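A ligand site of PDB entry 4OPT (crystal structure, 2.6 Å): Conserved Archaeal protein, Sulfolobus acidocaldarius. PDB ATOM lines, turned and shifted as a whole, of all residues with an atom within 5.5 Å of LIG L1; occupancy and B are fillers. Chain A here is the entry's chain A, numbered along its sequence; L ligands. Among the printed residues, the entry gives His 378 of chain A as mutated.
An oxygen (O4) of LIG L1 lies close to the backbone carbonyl oxygen (O) of Glu 93 (3.3 Å).
Residues that only touch LIG L1: His 298, Gly 92, Ala 55, Ala 51, Val 52, Trp 218, Tyr 216, Asn 91, Gly 300, Gly 299, Gly 94, Ile 77, Val 90, Phe 95 and Leu 203.
Within 4 Å of LIG L1: Ala 51, Val 52, Ser 53, Ala 55, Ile 77, Val 90, Asn 91, Gly 92, Glu 93, Gly 94, Phe 95, Leu 203, Tyr 216, Trp 218, His 298, Gly 299, Gly 300, His 378 and Glu 382.
The nearest printed residue that does not touch LIG L1 is Phe 220 (4.03 Å).
ND1 of His 378 lies close to O5 of LIG L1.
O of Ala 51 sits at hydrogen-bond distance from N7 of LG2 L2, 2.9 Å away.
An oxygen (O8) of LG2 L2 is in hydrogen-bond range of the backbone NH (N) of Ala 51, 3.3 Å away.
OE2 of Glu 382 lies close to O2 of LIG L1, at 3.1 Å.
An oxygen (O1) of LIG L1 lies within hydrogen-bond range of the side-chain hydroxyl of Ser 53 (3.0 Å).
O of Gly 92 is in hydrogen-bond range of N of Gly 76 (3.3 Å).
O of Asn 91 sits at hydrogen-bond distance from NE2 of His 378 (2.7 Å).
N of Gly 300 sits at hydrogen-bond distance from ND1 of His 298, at 2.9 Å.
The backbone NH (N) of Ala 55 is in hydrogen-bond range of the side-chain hydroxyl (OG) of Ser 53.
O of Asn 75 is in hydrogen-bond range of ND2 of Asn 91 (3.4 Å).
The backbone NH (N) of Gly 94 sits at hydrogen-bond distance from the backbone carbonyl oxygen (O) of Ile 74, at 2.9 Å.
N of Leu 203 is in hydrogen-bond range of O of Gly 76 (2.9 Å).
O of Val 52 is in hydrogen-bond range of N of Phe 95 (2.8 Å).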
ATOM      1  N   GLY A  49     -17.602   6.234  10.961  1.00  0.00           N
ATOM      2  CA  GLY A  49     -16.835   7.237  10.254  1.00  0.00           C
ATOM      3  C   GLY A  49     -16.329   6.692   8.937  1.00  0.00           C
ATOM      4  O   GLY A  49     -15.918   7.446   8.055  1.00  0.00           O
ATOM      5  N   ALA A  51     -13.676   5.257   8.226  1.00  0.00           N
ATOM      6  CA  ALA A  51     -12.255   5.514   8.001  1.00  0.00           C
ATOM      7  C   ALA A  51     -11.395   4.387   8.561  1.00  0.00           C
ATOM      8  O   ALA A  51     -11.367   4.153   9.776  1.00  0.00           O
ATOM      9  CB  ALA A  51     -11.853   6.837   8.626  1.00  0.00           C
ATOM     10  N   VAL A  52     -10.700   3.680   7.681  1.00  0.00           N
ATOM     11  CA  VAL A  52      -9.844   2.566   8.092  1.00  0.00           C
ATOM     12  C   VAL A  52      -8.435   2.716   7.512  1.00  0.00           C
ATOM     13  O   VAL A  52      -8.258   3.116   6.361  1.00  0.00           O
ATOM     14  CB  VAL A  52     -10.430   1.206   7.649  1.00  0.00           C
ATOM     15  CG1 VAL A  52      -9.646   0.062   8.272  1.00  0.00           C
ATOM     16  CG2 VAL A  52     -11.899   1.101   8.031  1.00  0.00           C
ATOM     17  N   SER A  53      -7.431   2.386   8.320  1.00  0.00           N
ATOM     18  CA  SER A  53      -6.034   2.420   7.884  1.00  0.00           C
ATOM     19  C   SER A  53      -5.747   1.345   6.838  1.00  0.00           C
ATOM     20  O   SER A  53      -6.338   0.271   6.864  1.00  0.00           O
ATOM     21  CB  SER A  53      -5.100   2.236   9.086  1.00  0.00           C
ATOM     22  OG  SER A  53      -3.762   2.046   8.671  1.00  0.00           O
ATOM     23  N   LYS A  54      -4.845   1.650   5.919  1.00  0.00           N
ATOM     24  CA  LYS A  54      -4.470   0.711   4.873  1.00  0.00           C
ATOM     25  C   LYS A  54      -3.618  -0.422   5.447  1.00  0.00           C
ATOM     26  O   LYS A  54      -3.646  -1.551   4.939  1.00  0.00           O
ATOM     27  CB  LYS A  54      -3.708   1.413   3.742  1.00  0.00           C
ATOM     28  CG  LYS A  54      -3.390   0.512   2.561  1.00  0.00           C
ATOM     29  CD  LYS A  54      -2.545   1.205   1.514  1.00  0.00           C
ATOM     30  CE  LYS A  54      -1.106   1.360   1.967  1.00  0.00           C
ATOM     31  NZ  LYS A  54      -0.228   1.849   0.862  1.00  0.00           N
ATOM     32  N   ALA A  55      -2.872  -0.118   6.500  1.00  0.00           N
ATOM     33  CA  ALA A  55      -1.963  -1.076   7.124  1.00  0.00           C
ATOM     34  C   ALA A  55      -2.702  -2.313   7.640  1.00  0.00           C
ATOM     35  O   ALA A  55      -2.144  -3.411   7.655  1.00  0.00           O
ATOM     36  CB  ALA A  55      -1.194  -0.416   8.251  1.00  0.00           C
ATOM     37  N   ILE A  74      -7.309   8.301   1.499  1.00  0.00           N
ATOM     38  CA  ILE A  74      -6.810   9.174   2.554  1.00  0.00           C
ATOM     39  C   ILE A  74      -5.284   9.132   2.622  1.00  0.00           C
ATOM     40  O   ILE A  74      -4.677   8.067   2.631  1.00  0.00           O
ATOM     41  CB  ILE A  74      -7.386   8.779   3.926  1.00  0.00           C
ATOM     42  CG1 ILE A  74      -8.913   8.835   3.892  1.00  0.00           C
ATOM     43  CG2 ILE A  74      -6.847   9.692   5.024  1.00  0.00           C
ATOM     44  CD1 ILE A  74      -9.472  10.165   3.436  1.00  0.00           C
ATOM     45  N   ASN A  75      -4.667  10.309   2.673  1.00  0.00           N
ATOM     46  CA  ASN A  75      -3.207  10.414   2.709  1.00  0.00           C
ATOM     47  C   ASN A  75      -2.680  10.976   4.034  1.00  0.00           C
ATOM     48  O   ASN A  75      -1.469  11.059   4.225  1.00  0.00           O
ATOM     49  CB  ASN A  75      -2.711  11.287   1.555  1.00  0.00           C
ATOM     50  CG  ASN A  75      -2.718  10.561   0.224  1.00  0.00           C
ATOM     51  OD1 ASN A  75      -2.423   9.365   0.162  1.00  0.00           O
ATOM     52  ND2 ASN A  75      -3.048  11.277  -0.843  1.00  0.00           N
ATOM     53  N   GLY A  76      -3.580  11.336   4.928  1.00  0.00           N
ATOM     54  CA  GLY A  76      -3.170  11.859   6.221  1.00  0.00           C
ATOM     55  C   GLY A  76      -4.295  12.435   7.059  1.00  0.00           C
ATOM     56  O   GLY A  76      -5.455  12.445   6.650  1.00  0.00           O
ATOM     57  N   ILE A  77      -3.943  12.911   8.251  1.00  0.00           N
ATOM     58  CA  ILE A  77      -4.920  13.482   9.180  1.00  0.00           C
ATOM     59  C   ILE A  77      -4.467  14.832   9.732  1.00  0.00           C
ATOM     60  O   ILE A  77      -3.378  14.941  10.304  1.00  0.00           O
ATOM     61  CB  ILE A  77      -5.191  12.536  10.373  1.00  0.00           C
ATOM     62  CG1 ILE A  77      -5.678  11.173   9.888  1.00  0.00           C
ATOM     63  CG2 ILE A  77      -6.193  13.153  11.328  1.00  0.00           C
ATOM     64  CD1 ILE A  77      -5.890  10.173  11.007  1.00  0.00           C
ATOM     65  N   VAL A  90      -0.550  14.546  10.378  1.00  0.00           N
ATOM     66  CA  VAL A  90      -0.005  13.196  10.467  1.00  0.00           C
ATOM     67  C   VAL A  90      -0.228  12.437   9.168  1.00  0.00           C
ATOM     68  O   VAL A  90      -1.371  12.136   8.803  1.00  0.00           O
ATOM     69  CB  VAL A  90      -0.636  12.406  11.632  1.00  0.00           C
ATOM     70  CG1 VAL A  90      -0.061  10.997  11.691  1.00  0.00           C
ATOM     71  CG2 VAL A  90      -0.417  13.135  12.951  1.00  0.00           C
ATOM     72  N   ASN A  91       0.857  12.129   8.463  1.00  0.00           N
ATOM     73  CA  ASN A  91       0.759  11.436   7.185  1.00  0.00           C
ATOM     74  C   ASN A  91       0.647   9.919   7.322  1.00  0.00           C
ATOM     75  O   ASN A  91       1.247   9.325   8.225  1.00  0.00           O
ATOM     76  CB  ASN A  91       1.962  11.787   6.299  1.00  0.00           C
ATOM     77  CG  ASN A  91       1.780  13.096   5.564  1.00  0.00           C
ATOM     78  OD1 ASN A  91       2.039  14.170   6.111  1.00  0.00           O
ATOM     79  ND2 ASN A  91       1.328  13.021   4.317  1.00  0.00           N
ATOM     80  N   GLY A  92      -0.130   9.311   6.433  1.00  0.00           N
ATOM     81  CA  GLY A  92      -0.357   7.880   6.442  1.00  0.00           C
ATOM     82  C   GLY A  92      -1.515   7.536   5.524  1.00  0.00           C
ATOM     83  O   GLY A  92      -2.475   8.291   5.432  1.00  0.00           O
ATOM     84  N   GLU A  93      -1.411   6.402   4.841  1.00  0.00           N
ATOM     85  CA  GLU A  93      -2.432   6.017   3.872  1.00  0.00           C
ATOM     86  C   GLU A  93      -3.592   5.271   4.532  1.00  0.00           C
ATOM     87  O   GLU A  93      -3.394   4.436   5.412  1.00  0.00           O
ATOM     88  CB  GLU A  93      -1.807   5.151   2.774  1.00  0.00           C
ATOM     89  CG  GLU A  93      -0.672   5.826   2.029  1.00  0.00           C
ATOM     90  CD  GLU A  93      -0.168   5.007   0.856  1.00  0.00           C
ATOM     91  OE1 GLU A  93       1.064   4.956   0.664  1.00  0.00           O
ATOM     92  OE2 GLU A  93      -0.999   4.424   0.134  1.00  0.00           O
ATOM     93  N   GLY A  94      -4.804   5.599   4.104  1.00  0.00           N
ATOM     94  CA  GLY A  94      -6.002   4.968   4.619  1.00  0.00           C
ATOM     95  C   GLY A  94      -7.136   5.024   3.605  1.00  0.00           C
ATOM     96  O   GLY A  94      -6.944   5.496   2.490  1.00  0.00           O
ATOM     97  N   PHE A  95      -8.311   4.539   3.996  1.00  0.00           N
ATOM     98  CA  PHE A  95      -9.448   4.505   3.093  1.00  0.00           C
ATOM     99  C   PHE A  95     -10.726   5.045   3.718  1.00  0.00           C
ATOM    100  O   PHE A  95     -11.075   4.708   4.849  1.00  0.00           O
ATOM    101  CB  PHE A  95      -9.715   3.067   2.617  1.00  0.00           C
ATOM    102  CG  PHE A  95      -8.521   2.400   1.991  1.00  0.00           C
ATOM    103  CD1 PHE A  95      -8.004   2.854   0.792  1.00  0.00           C
ATOM    104  CD2 PHE A  95      -7.941   1.300   2.594  1.00  0.00           C
ATOM    105  CE1 PHE A  95      -6.919   2.238   0.217  1.00  0.00           C
ATOM    106  CE2 PHE A  95      -6.851   0.671   2.016  1.00  0.00           C
ATOM    107  CZ  PHE A  95      -6.338   1.139   0.820  1.00  0.00           C
ATOM    108  N   ALA A 186     -21.341   8.118  20.015  1.00  0.00           N
ATOM    109  CA  ALA A 186     -20.892   8.857  18.844  1.00  0.00           C
ATOM    110  C   ALA A 186     -22.023   8.987  17.815  1.00  0.00           C
ATOM    111  O   ALA A 186     -22.826   8.081  17.656  1.00  0.00           O
ATOM    112  CB  ALA A 186     -19.687   8.185  18.223  1.00  0.00           C
ATOM    113  N   LEU A 203      -8.065  13.758   6.501  1.00  0.00           N
ATOM    114  CA  LEU A 203      -9.093  13.757   7.539  1.00  0.00           C
ATOM    115  C   LEU A 203      -8.866  14.917   8.490  1.00  0.00           C
ATOM    116  O   LEU A 203      -7.745  15.389   8.665  1.00  0.00           O
ATOM    117  CB  LEU A 203      -9.082  12.427   8.310  1.00  0.00           C
ATOM    118  CG  LEU A 203      -9.308  11.145   7.508  1.00  0.00           C
ATOM    119  CD1 LEU A 203      -9.319   9.934   8.422  1.00  0.00           C
ATOM    120  CD2 LEU A 203     -10.600  11.241   6.706  1.00  0.00           C
ATOM    121  N   ILE A 205      -9.611  16.259  12.490  1.00  0.00           N
ATOM    122  CA  ILE A 205     -10.024  15.944  13.847  1.00  0.00           C
ATOM    123  C   ILE A 205      -9.911  17.173  14.744  1.00  0.00           C
ATOM    124  O   ILE A 205      -8.846  17.784  14.838  1.00  0.00           O
ATOM    125  CB  ILE A 205      -9.197  14.791  14.440  1.00  0.00           C
ATOM    126  CG1 ILE A 205      -9.544  13.472  13.749  1.00  0.00           C
ATOM    127  CG2 ILE A 205      -9.429  14.669  15.938  1.00  0.00           C
ATOM    128  CD1 ILE A 205      -8.789  12.279  14.280  1.00  0.00           C
ATOM    129  N   TYR A 216     -14.032  13.941  20.559  1.00  0.00           N
ATOM    130  CA  TYR A 216     -13.645  14.962  19.588  1.00  0.00           C
ATOM    131  C   TYR A 216     -14.645  15.058  18.436  1.00  0.00           C
ATOM    132  O   TYR A 216     -15.531  14.222  18.285  1.00  0.00           O
ATOM    133  CB  TYR A 216     -12.245  14.680  19.039  1.00  0.00           C
ATOM    134  CG  TYR A 216     -12.089  13.347  18.333  1.00  0.00           C
ATOM    135  CD1 TYR A 216     -12.440  13.199  16.993  1.00  0.00           C
ATOM    136  CD2 TYR A 216     -11.567  12.244  18.994  1.00  0.00           C
ATOM    137  CE1 TYR A 216     -12.287  11.980  16.345  1.00  0.00           C
ATOM    138  CE2 TYR A 216     -11.410  11.025  18.355  1.00  0.00           C
ATOM    139  CZ  TYR A 216     -11.778  10.907  17.025  1.00  0.00           C
ATOM    140  OH  TYR A 216     -11.629   9.702  16.380  1.00  0.00           O
ATOM    141  N   TRP A 218     -15.047  15.306  14.155  1.00  0.00           N
ATOM    142  CA  TRP A 218     -14.301  14.906  12.972  1.00  0.00           C
ATOM    143  C   TRP A 218     -14.945  15.372  11.670  1.00  0.00           C
ATOM    144  O   TRP A 218     -16.169  15.542  11.578  1.00  0.00           O
ATOM    145  CB  TRP A 218     -14.106  13.385  12.948  1.00  0.00           C
ATOM    146  CG  TRP A 218     -15.331  12.567  12.647  1.00  0.00           C
ATOM    147  CD1 TRP A 218     -15.885  12.331  11.424  1.00  0.00           C
ATOM    148  CD2 TRP A 218     -16.141  11.851  13.589  1.00  0.00           C
ATOM    149  NE1 TRP A 218     -16.988  11.532  11.542  1.00  0.00           N
ATOM    150  CE2 TRP A 218     -17.175  11.225  12.860  1.00  0.00           C
ATOM    151  CE3 TRP A 218     -16.107  11.692  14.973  1.00  0.00           C
ATOM    152  CZ2 TRP A 218     -18.146  10.437  13.480  1.00  0.00           C
ATOM    153  CZ3 TRP A 218     -17.077  10.914  15.583  1.00  0.00           C
ATOM    154  CH2 TRP A 218     -18.091  10.300  14.835  1.00  0.00           C
ATOM    155  N   PHE A 220     -14.537  13.993   7.990  1.00  0.00           N
ATOM    156  CA  PHE A 220     -13.974  12.983   7.109  1.00  0.00           C
ATOM    157  C   PHE A 220     -14.562  13.065   5.696  1.00  0.00           C
ATOM    158  O   PHE A 220     -15.707  12.667   5.475  1.00  0.00           O
ATOM    159  CB  PHE A 220     -14.218  11.575   7.672  1.00  0.00           C
ATOM    160  CG  PHE A 220     -13.457  11.286   8.945  1.00  0.00           C
ATOM    161  CD1 PHE A 220     -12.533  12.185   9.446  1.00  0.00           C
ATOM    162  CD2 PHE A 220     -13.682  10.098   9.635  1.00  0.00           C
ATOM    163  CE1 PHE A 220     -11.842  11.898  10.618  1.00  0.00           C
ATOM    164  CE2 PHE A 220     -12.995   9.812  10.798  1.00  0.00           C
ATOM    165  CZ  PHE A 220     -12.075  10.712  11.290  1.00  0.00           C
ATOM    166  N   VAL A 270     -19.808   3.295  21.403  1.00  0.00           N
ATOM    167  CA  VAL A 270     -18.438   2.899  21.060  1.00  0.00           C
ATOM    168  C   VAL A 270     -17.635   2.567  22.311  1.00  0.00           C
ATOM    169  O   VAL A 270     -17.395   3.440  23.148  1.00  0.00           O
ATOM    170  CB  VAL A 270     -17.699   4.008  20.290  1.00  0.00           C
ATOM    171  CG1 VAL A 270     -16.295   3.541  19.936  1.00  0.00           C
ATOM    172  CG2 VAL A 270     -18.454   4.394  19.036  1.00  0.00           C
ATOM    173  N   HIS A 298      -8.570   6.984  19.745  1.00  0.00           N
ATOM    174  CA  HIS A 298      -9.225   7.641  18.610  1.00  0.00           C
ATOM    175  C   HIS A 298     -10.534   6.963  18.219  1.00  0.00           C
ATOM    176  O   HIS A 298     -11.243   7.442  17.326  1.00  0.00           O
ATOM    177  CB  HIS A 298      -8.275   7.719  17.407  1.00  0.00           C
ATOM    178  CG  HIS A 298      -7.766   6.389  16.937  1.00  0.00           C
ATOM    179  ND1 HIS A 298      -8.579   5.418  16.414  1.00  0.00           N
ATOM    180  CD2 HIS A 298      -6.498   5.894  16.887  1.00  0.00           C
ATOM    181  CE1 HIS A 298      -7.856   4.365  16.071  1.00  0.00           C
ATOM    182  NE2 HIS A 298      -6.588   4.627  16.357  1.00  0.00           N
ATOM    183  N   GLY A 299     -10.865   5.851  18.863  1.00  0.00           N
ATOM    184  CA  GLY A 299     -12.157   5.213  18.675  1.00  0.00           C
ATOM    185  C   GLY A 299     -12.291   4.353  17.436  1.00  0.00           C
ATOM    186  O   GLY A 299     -13.400   3.919  17.097  1.00  0.00           O
ATOM    187  N   GLY A 300     -11.182   4.102  16.750  1.00  0.00           N
ATOM    188  CA  GLY A 300     -11.200   3.250  15.572  1.00  0.00           C
ATOM    189  C   GLY A 300     -11.279   1.790  15.952  1.00  0.00           C
ATOM    190  O   GLY A 300     -10.473   1.293  16.737  1.00  0.00           O
ATOM    191  N   HIS A 378       3.304   9.144  15.886  1.00  0.00           N
ATOM    192  CA  HIS A 378       3.102   7.949  15.073  1.00  0.00           C
ATOM    193  C   HIS A 378       3.384   6.702  15.904  1.00  0.00           C
ATOM    194  O   HIS A 378       2.660   5.713  15.843  1.00  0.00           O
ATOM    195  CB  HIS A 378       4.013   7.977  13.837  1.00  0.00           C
ATOM    196  CG  HIS A 378       3.269   8.159  12.555  1.00  0.00           C
ATOM    197  ND1 HIS A 378       2.582   7.137  11.942  1.00  0.00           N
ATOM    198  CD2 HIS A 378       3.127   9.238  11.756  1.00  0.00           C
ATOM    199  CE1 HIS A 378       2.040   7.582  10.824  1.00  0.00           C
ATOM    200  NE2 HIS A 378       2.350   8.859  10.686  1.00  0.00           N
ATOM    201  N   GLU A 382       0.064   3.593  17.414  1.00  0.00           N
ATOM    202  CA  GLU A 382       0.265   2.468  16.517  1.00  0.00           C
ATOM    203  C   GLU A 382       0.945   1.311  17.237  1.00  0.00           C
ATOM    204  O   GLU A 382       0.816   0.158  16.844  1.00  0.00           O
ATOM    205  CB  GLU A 382       1.073   2.880  15.291  1.00  0.00           C
ATOM    206  CG  GLU A 382       0.295   3.710  14.282  1.00  0.00           C
ATOM    207  CD  GLU A 382       1.034   3.906  12.973  1.00  0.00           C
ATOM    208  OE1 GLU A 382       2.288   3.893  12.994  1.00  0.00           O
ATOM    209  OE2 GLU A 382       0.374   4.079  11.928  1.00  0.00           O
HETATM  210  C1  LIG L   1     -14.464   8.729  14.391  1.00  0.00           C
HETATM  211  C2  LIG L   1     -15.050   7.076  16.343  1.00  0.00           C
HETATM  212  C3  LIG L   1     -14.130   7.513  15.225  1.00  0.00           C
HETATM  213  C4  LIG L   1     -13.005   6.825  14.962  1.00  0.00           C
HETATM  214  C5  LIG L   1     -12.090   7.275  13.848  1.00  0.00           C
HETATM  215  C6  LIG L   1      -9.229   8.184  13.218  1.00  0.00           C
HETATM  216  C7  LIG L   1      -9.879   6.866  12.827  1.00  0.00           C
HETATM  217  C8  LIG L   1     -10.973   6.268  13.684  1.00  0.00           C
HETATM  218  C9  LIG L   1      -9.508   6.219  11.708  1.00  0.00           C
HETATM  219  C10 LIG L   1      -8.429   6.776  10.809  1.00  0.00           C
HETATM  220  C11 LIG L   1      -7.979   5.661   9.897  1.00  0.00           C
HETATM  221  C12 LIG L   1      -7.238   6.225   8.705  1.00  0.00           C
HETATM  222  C13 LIG L   1      -7.943   6.365   7.370  1.00  0.00           C
HETATM  223  C14 LIG L   1      -5.964   6.607   8.860  1.00  0.00           C
HETATM  224  C15 LIG L   1      -5.159   7.190   7.709  1.00  0.00           C
HETATM  225  C16 LIG L   1      -4.113   8.156   8.222  1.00  0.00           C
HETATM  226  C17 LIG L   1      -3.101   7.490   9.130  1.00  0.00           C
HETATM  227  C18 LIG L   1      -2.384   8.321  10.178  1.00  0.00           C
HETATM  228  C19 LIG L   1      -2.840   6.164   9.024  1.00  0.00           C
HETATM  229  C20 LIG L   1      -1.852   5.487   9.942  1.00  0.00           C
HETATM  230  O1  LIG L   1      -1.770   4.133   9.559  1.00  0.00           O
HETATM  231  P1  LIG L   1      -0.485   3.698   8.768  1.00  0.00           P
HETATM  232  O2  LIG L   1       0.065   2.415   9.364  1.00  0.00           O
HETATM  233  O3  LIG L   1       0.586   4.847   8.920  1.00  0.00           O
HETATM  234  O4  LIG L   1      -0.827   3.484   7.307  1.00  0.00           O
HETATM  235  P2  LIG L   1       2.039   4.800   8.299  1.00  0.00           P
HETATM  236  O5  LIG L   1       3.051   4.784   9.423  1.00  0.00           O
HETATM  237  O6  LIG L   1       2.194   3.545   7.462  1.00  0.00           O
HETATM  238  O7  LIG L   1       2.261   6.021   7.441  1.00  0.00           O
HETATM  239  P1  LG2 L   2     -21.187  -4.270  14.001  1.00  0.00           P
HETATM  240  O1  LG2 L   2     -22.183  -3.596  14.862  1.00  0.00           O
HETATM  241  O2  LG2 L   2     -20.985  -3.623  12.629  1.00  0.00           O
HETATM  242  O3  LG2 L   2     -21.582  -5.799  13.906  1.00  0.00           O
HETATM  243  C1  LG2 L   2     -22.828  -6.264  14.459  1.00  0.00           C
HETATM  244  C2  LG2 L   2     -23.569  -7.051  13.416  1.00  0.00           C
HETATM  245  O4  LG2 L   2     -24.152  -8.230  14.026  1.00  0.00           O
HETATM  246  C3  LG2 L   2     -24.728  -6.315  12.740  1.00  0.00           C
HETATM  247  O5  LG2 L   2     -24.798  -6.634  11.350  1.00  0.00           O
HETATM  248  C4  LG2 L   2     -25.947  -6.809  13.507  1.00  0.00           C
HETATM  249  O6  LG2 L   2     -27.125  -6.775  12.705  1.00  0.00           O
HETATM  250  C5  LG2 L   2     -25.554  -8.253  13.801  1.00  0.00           C
HETATM  251  N1  LG2 L   2     -26.200  -8.840  14.962  1.00  0.00           N
HETATM  252  C6  LG2 L   2     -26.247  -8.325  16.238  1.00  0.00           C
HETATM  253  N2  LG2 L   2     -26.903  -9.070  17.102  1.00  0.00           N
HETATM  254  C7  LG2 L   2     -27.319 -10.146  16.326  1.00  0.00           C
HETATM  255  C8  LG2 L   2     -28.073 -11.302  16.651  1.00  0.00           C
HETATM  256  N3  LG2 L   2     -28.540 -11.570  17.871  1.00  0.00           N
HETATM  257  N4  LG2 L   2     -28.312 -12.187  15.649  1.00  0.00           N
HETATM  258  C9  LG2 L   2     -27.846 -11.919  14.429  1.00  0.00           C
HETATM  259  N5  LG2 L   2     -27.125 -10.875  14.018  1.00  0.00           N
HETATM  260  C10 LG2 L   2     -26.897 -10.018  15.021  1.00  0.00           C
HETATM  261  N6  LG2 L   2     -14.208   2.536  13.389  1.00  0.00           N
HETATM  262  C11 LG2 L   2     -13.118   2.823  12.609  1.00  0.00           C
HETATM  263  O7  LG2 L   2     -12.276   1.974  12.337  1.00  0.00           O
HETATM  264  N7  LG2 L   2     -13.026   4.118  12.139  1.00  0.00           N
HETATM  265  C12 LG2 L   2     -14.023   5.060  12.138  1.00  0.00           C
HETATM  266  O8  LG2 L   2     -13.961   6.030  11.372  1.00  0.00           O
HETATM  267  C13 LG2 L   2     -15.045   4.765  13.074  1.00  0.00           C
HETATM  268  N8  LG2 L   2     -15.962   5.726  13.379  1.00  0.00           N
HETATM  269  C14 LG2 L   2     -17.107   5.393  14.090  1.00  0.00           C
HETATM  270  C15 LG2 L   2     -18.181   6.278  14.213  1.00  0.00           C
HETATM  271  C16 LG2 L   2     -19.330   5.946  14.915  1.00  0.00           C
HETATM  272  C17 LG2 L   2     -20.465   6.932  14.986  1.00  0.00           C
HETATM  273  C18 LG2 L   2     -19.426   4.685  15.520  1.00  0.00           C
HETATM  274  C19 LG2 L   2     -20.654   4.281  16.279  1.00  0.00           C
HETATM  275  C20 LG2 L   2     -18.353   3.801  15.420  1.00  0.00           C
HETATM  276  C21 LG2 L   2     -17.208   4.134  14.709  1.00  0.00           C
HETATM  277  N9  LG2 L   2     -16.121   3.253  14.582  1.00  0.00           N
HETATM  278  C22 LG2 L   2     -15.117   3.526  13.683  1.00  0.00           C
HETATM  279  C23 LG2 L   2     -16.160   1.913  15.209  1.00  0.00           C
HETATM  280  C24 LG2 L   2     -16.672   0.865  14.226  1.00  0.00           C
HETATM  281  O9  LG2 L   2     -17.883   1.322  13.617  1.00  0.00           O
HETATM  282  C25 LG2 L   2     -16.935  -0.446  14.961  1.00  0.00           C
HETATM  283  O10 LG2 L   2     -15.972  -0.588  16.003  1.00  0.00           O
HETATM  284  C26 LG2 L   2     -16.872  -1.686  14.065  1.00  0.00           C
HETATM  285  O11 LG2 L   2     -17.888  -1.594  13.061  1.00  0.00           O
HETATM  286  C27 LG2 L   2     -16.993  -2.968  14.842  1.00  0.00           C
HETATM  287  O12 LG2 L   2     -17.406  -4.031  13.958  1.00  0.00           O
HETATM  288  P2  LG2 L   2     -18.447  -5.125  14.453  1.00  0.00           P
HETATM  289  O13 LG2 L   2     -18.671  -6.078  13.349  1.00  0.00           O
HETATM  290  O14 LG2 L   2     -18.060  -5.760  15.788  1.00  0.00           O
HETATM  291  O15 LG2 L   2     -19.766  -4.264  14.718  1.00  0.00           O
